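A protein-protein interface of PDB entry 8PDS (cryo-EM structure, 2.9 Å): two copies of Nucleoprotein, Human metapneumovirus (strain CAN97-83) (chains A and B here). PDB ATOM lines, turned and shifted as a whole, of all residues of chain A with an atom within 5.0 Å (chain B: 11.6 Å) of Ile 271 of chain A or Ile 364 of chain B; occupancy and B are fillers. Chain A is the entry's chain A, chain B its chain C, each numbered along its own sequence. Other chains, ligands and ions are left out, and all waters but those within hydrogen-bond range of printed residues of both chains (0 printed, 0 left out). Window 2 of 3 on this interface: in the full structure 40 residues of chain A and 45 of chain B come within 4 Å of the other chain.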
ATOM      1  N   ASN A 269      -5.796  31.535  36.678  1.00  0.00           N
ATOM      2  CA  ASN A 269      -5.027  31.689  35.443  1.00  0.00           C
ATOM      3  C   ASN A 269      -3.749  30.858  35.478  1.00  0.00           C
ATOM      4  O   ASN A 269      -2.685  31.303  35.045  1.00  0.00           O
ATOM      5  CB  ASN A 269      -4.706  33.160  35.164  1.00  0.00           C
ATOM      6  CG  ASN A 269      -5.950  34.006  34.988  1.00  0.00           C
ATOM      7  OD1 ASN A 269      -6.856  33.653  34.232  1.00  0.00           O
ATOM      8  ND2 ASN A 269      -5.997  35.136  35.683  1.00  0.00           N
ATOM      9  N   ASN A 270      -3.852  29.641  36.006  1.00  0.00           N
ATOM     10  CA  ASN A 270      -2.706  28.745  36.058  1.00  0.00           C
ATOM     11  C   ASN A 270      -2.256  28.401  34.646  1.00  0.00           C
ATOM     12  O   ASN A 270      -3.011  27.800  33.878  1.00  0.00           O
ATOM     13  CB  ASN A 270      -3.072  27.480  36.831  1.00  0.00           C
ATOM     14  CG  ASN A 270      -1.871  26.806  37.456  1.00  0.00           C
ATOM     15  OD1 ASN A 270      -1.134  27.416  38.224  1.00  0.00           O
ATOM     16  ND2 ASN A 270      -1.673  25.538  37.135  1.00  0.00           N
ATOM     17  N   ILE A 271      -1.022  28.781  34.300  1.00  0.00           N
ATOM     18  CA  ILE A 271      -0.566  28.606  32.927  1.00  0.00           C
ATOM     19  C   ILE A 271      -0.264  27.152  32.612  1.00  0.00           C
ATOM     20  O   ILE A 271      -0.167  26.787  31.437  1.00  0.00           O
ATOM     21  CB  ILE A 271       0.676  29.462  32.627  1.00  0.00           C
ATOM     22  CG1 ILE A 271       1.844  29.041  33.515  1.00  0.00           C
ATOM     23  CG2 ILE A 271       0.361  30.934  32.811  1.00  0.00           C
ATOM     24  CD1 ILE A 271       3.159  29.671  33.121  1.00  0.00           C
ATOM     25  N   MET A 272      -0.101  26.304  33.628  1.00  0.00           N
ATOM     26  CA  MET A 272       0.077  24.888  33.353  1.00  0.00           C
ATOM     27  C   MET A 272      -1.200  24.237  32.848  1.00  0.00           C
ATOM     28  O   MET A 272      -1.155  23.086  32.402  1.00  0.00           O
ATOM     29  CB  MET A 272       0.582  24.162  34.597  1.00  0.00           C
ATOM     30  CG  MET A 272       1.920  24.668  35.099  1.00  0.00           C
ATOM     31  SD  MET A 272       3.196  24.682  33.830  1.00  0.00           S
ATOM     32  CE  MET A 272       3.223  22.960  33.357  1.00  0.00           C
ATOM     33  N   LEU A 273      -2.333  24.938  32.917  1.00  0.00           N
ATOM     34  CA  LEU A 273      -3.524  24.505  32.203  1.00  0.00           C
ATOM     35  C   LEU A 273      -3.322  24.550  30.697  1.00  0.00           C
ATOM     36  O   LEU A 273      -4.015  23.832  29.968  1.00  0.00           O
ATOM     37  CB  LEU A 273      -4.719  25.374  32.593  1.00  0.00           C
ATOM     38  CG  LEU A 273      -5.300  25.163  33.990  1.00  0.00           C
ATOM     39  CD1 LEU A 273      -6.400  26.166  34.252  1.00  0.00           C
ATOM     40  CD2 LEU A 273      -5.821  23.747  34.150  1.00  0.00           C
ATOM     41  N   GLY A 274      -2.394  25.378  30.218  1.00  0.00           N
ATOM     42  CA  GLY A 274      -2.028  25.448  28.823  1.00  0.00           C
ATOM     43  C   GLY A 274      -1.073  24.376  28.363  1.00  0.00           C
ATOM     44  O   GLY A 274      -0.704  24.346  27.188  1.00  0.00           O
ATOM     45  N   HIS A 275      -0.655  23.498  29.267  1.00  0.00           N
ATOM     46  CA  HIS A 275       0.173  22.363  28.895  1.00  0.00           C
ATOM     47  C   HIS A 275      -0.602  21.435  27.965  1.00  0.00           C
ATOM     48  O   HIS A 275      -1.814  21.259  28.100  1.00  0.00           O
ATOM     49  CB  HIS A 275       0.616  21.616  30.152  1.00  0.00           C
ATOM     50  CG  HIS A 275       1.732  20.649  29.927  1.00  0.00           C
ATOM     51  ND1 HIS A 275       1.517  19.339  29.558  1.00  0.00           N
ATOM     52  CD2 HIS A 275       3.073  20.793  30.040  1.00  0.00           C
ATOM     53  CE1 HIS A 275       2.678  18.720  29.444  1.00  0.00           C
ATOM     54  NE2 HIS A 275       3.639  19.581  29.731  1.00  0.00           N
ATOM     55  N   TYR A 354       4.013  27.720  40.017  1.00  0.00           N
ATOM     56  CA  TYR A 354       3.351  28.882  39.434  1.00  0.00           C
ATOM     57  C   TYR A 354       2.337  29.480  40.398  1.00  0.00           C
ATOM     58  O   TYR A 354       2.217  30.705  40.494  1.00  0.00           O
ATOM     59  CB  TYR A 354       2.685  28.517  38.107  1.00  0.00           C
ATOM     60  CG  TYR A 354       1.952  29.677  37.466  1.00  0.00           C
ATOM     61  CD1 TYR A 354       0.635  29.971  37.800  1.00  0.00           C
ATOM     62  CD2 TYR A 354       2.595  30.511  36.563  1.00  0.00           C
ATOM     63  CE1 TYR A 354      -0.029  31.038  37.227  1.00  0.00           C
ATOM     64  CE2 TYR A 354       1.940  31.582  35.988  1.00  0.00           C
ATOM     65  CZ  TYR A 354       0.629  31.839  36.324  1.00  0.00           C
ATOM     66  OH  TYR A 354      -0.029  32.904  35.755  1.00  0.00           O
ATOM     67  N   LEU B 358       5.847  13.308  20.861  1.00  0.00           N
ATOM     68  CA  LEU B 358       4.932  14.270  21.462  1.00  0.00           C
ATOM     69  C   LEU B 358       4.810  14.057  22.966  1.00  0.00           C
ATOM     70  O   LEU B 358       4.788  15.024  23.735  1.00  0.00           O
ATOM     71  CB  LEU B 358       3.568  14.177  20.777  1.00  0.00           C
ATOM     72  CG  LEU B 358       2.472  15.195  21.098  1.00  0.00           C
ATOM     73  CD1 LEU B 358       1.542  15.327  19.910  1.00  0.00           C
ATOM     74  CD2 LEU B 358       1.670  14.783  22.324  1.00  0.00           C
ATOM     75  N   LYS B 359       4.722  12.801  23.403  1.00  0.00           N
ATOM     76  CA  LYS B 359       4.553  12.527  24.827  1.00  0.00           C
ATOM     77  C   LYS B 359       5.805  12.892  25.614  1.00  0.00           C
ATOM     78  O   LYS B 359       5.709  13.421  26.727  1.00  0.00           O
ATOM     79  CB  LYS B 359       4.182  11.058  25.036  1.00  0.00           C
ATOM     80  CG  LYS B 359       4.236  10.591  26.479  1.00  0.00           C
ATOM     81  CD  LYS B 359       4.059   9.084  26.578  1.00  0.00           C
ATOM     82  CE  LYS B 359       5.287   8.346  26.077  1.00  0.00           C
ATOM     83  NZ  LYS B 359       5.181   6.878  26.303  1.00  0.00           N
ATOM     84  N   GLU B 360       6.989  12.623  25.056  1.00  0.00           N
ATOM     85  CA  GLU B 360       8.223  12.927  25.776  1.00  0.00           C
ATOM     86  C   GLU B 360       8.390  14.426  26.001  1.00  0.00           C
ATOM     87  O   GLU B 360       8.770  14.858  27.095  1.00  0.00           O
ATOM     88  CB  GLU B 360       9.429  12.362  25.028  1.00  0.00           C
ATOM     89  CG  GLU B 360       9.469  10.846  24.969  1.00  0.00           C
ATOM     90  CD  GLU B 360       9.677  10.219  26.332  1.00  0.00           C
ATOM     91  OE1 GLU B 360      10.357  10.840  27.175  1.00  0.00           O
ATOM     92  OE2 GLU B 360       9.160   9.105  26.559  1.00  0.00           O
ATOM     93  N   SER B 361       8.107  15.235  24.984  1.00  0.00           N
ATOM     94  CA  SER B 361       8.305  16.670  25.103  1.00  0.00           C
ATOM     95  C   SER B 361       7.127  17.324  25.820  1.00  0.00           C
ATOM     96  O   SER B 361       6.025  16.775  25.900  1.00  0.00           O
ATOM     97  CB  SER B 361       8.496  17.306  23.727  1.00  0.00           C
ATOM     98  OG  SER B 361       9.489  16.621  22.982  1.00  0.00           O
ATOM     99  N   ASN B 362       7.378  18.521  26.347  1.00  0.00           N
ATOM    100  CA  ASN B 362       6.368  19.307  27.040  1.00  0.00           C
ATOM    101  C   ASN B 362       6.303  20.701  26.434  1.00  0.00           C
ATOM    102  O   ASN B 362       7.335  21.341  26.213  1.00  0.00           O
ATOM    103  CB  ASN B 362       6.664  19.397  28.543  1.00  0.00           C
ATOM    104  CG  ASN B 362       8.121  19.696  28.837  1.00  0.00           C
ATOM    105  OD1 ASN B 362       8.933  19.847  27.925  1.00  0.00           O
ATOM    106  ND2 ASN B 362       8.458  19.782  30.118  1.00  0.00           N
ATOM    107  N   LYS B 363       5.085  21.165  26.166  1.00  0.00           N
ATOM    108  CA  LYS B 363       4.869  22.472  25.566  1.00  0.00           C
ATOM    109  C   LYS B 363       3.714  23.163  26.274  1.00  0.00           C
ATOM    110  O   LYS B 363       2.840  22.517  26.858  1.00  0.00           O
ATOM    111  CB  LYS B 363       4.577  22.366  24.062  1.00  0.00           C
ATOM    112  CG  LYS B 363       5.729  21.820  23.238  1.00  0.00           C
ATOM    113  CD  LYS B 363       6.912  22.772  23.233  1.00  0.00           C
ATOM    114  CE  LYS B 363       8.083  22.190  22.458  1.00  0.00           C
ATOM    115  NZ  LYS B 363       9.256  23.107  22.450  1.00  0.00           N
ATOM    116  N   ILE B 364       3.717  24.492  26.214  1.00  0.00           N
ATOM    117  CA  ILE B 364       2.679  25.317  26.819  1.00  0.00           C
ATOM    118  C   ILE B 364       2.000  26.113  25.715  1.00  0.00           C
ATOM    119  O   ILE B 364       2.671  26.778  24.919  1.00  0.00           O
ATOM    120  CB  ILE B 364       3.252  26.255  27.896  1.00  0.00           C
ATOM    121  CG1 ILE B 364       4.087  25.466  28.904  1.00  0.00           C
ATOM    122  CG2 ILE B 364       2.131  26.993  28.608  1.00  0.00           C
ATOM    123  CD1 ILE B 364       3.278  24.513  29.742  1.00  0.00           C
ATOM    124  N   ASN B 365       0.673  26.044  25.671  1.00  0.00           N
ATOM    125  CA  ASN B 365      -0.097  26.771  24.670  1.00  0.00           C
ATOM    126  C   ASN B 365      -0.554  28.123  25.207  1.00  0.00           C
ATOM    127  O   ASN B 365      -1.493  28.724  24.684  1.00  0.00           O
ATOM    128  CB  ASN B 365      -1.303  25.946  24.220  1.00  0.00           C
ATOM    129  CG  ASN B 365      -0.907  24.736  23.399  1.00  0.00           C
ATOM    130  OD1 ASN B 365      -1.458  23.648  23.568  1.00  0.00           O
ATOM    131  ND2 ASN B 365       0.056  24.919  22.504  1.00  0.00           N
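O of Gly 274 of chain A lies within hydrogen-bond range of N of Asn 365 of chain B (2.7 Å).
Ile 364 of chain B touches Ile 271 of chain A.
Met 272 of chain A touches Ile 364 of chain B.
Ile 364 of chain B touches Gly 274 of chain A.
Asn 362 of chain B touches His 275 of chain A.
His 275 of chain A touches Lys 363 of chain B.
His 275 of chain A touches Ile 364 of chain B.
Ile 364 of chain B touches four residues of chain A.
Met 272 of chain A touches just one residue of chain B: Ile 364.
No residue of chain B comes within 4 Å of Leu 273 of chain A.
Of chain B, only Asn 362, Lys 363 and Ile 364 come within 4 Å of His 275 of chain A.
No residue of chain B comes within 4 Å of Tyr 354 of chain A.
Printed residues of chain B within 4 Å of Gly 274 of chain A: Ile 364 (3.5 Å) and Asn 365 (2.7 Å).
Of the printed residues of chain A, Lys 363 of chain B touches His 275 (3.4 Å).
Of the printed residues of chain A, Asn 365 of chain B touches Gly 274 (2.7 Å).
Of the printed residues of chain A, Asn 362 of chain B touches His 275 (3.3 Å).
Lys 359 of chain B touches none of the printed residues of chain A.
Leu 358 of chain B touches none of the printed residues of chain A.
The nearest printed residue of chain A that does not touch Lys 363 of chain B is Gly 274 of chain A (4.002 Å).
Of the 8 printed residues of chain A, 4 touch a printed residue of chain B.
Along chain A the printed residues that touch a printed residue of chain B span positions 271 to 275.
Hydrophobic or aromatic side chains of chain B within 4 Å of the printed part of chain A: Ile 364.
Among the printed residues, 7 pairs touch across the chains.
Among the printed residues, no Asp or Glu carboxylate lies within 4 Å of a Lys or Arg side-chain nitrogen of the other chain.
No position is printed for both chains.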
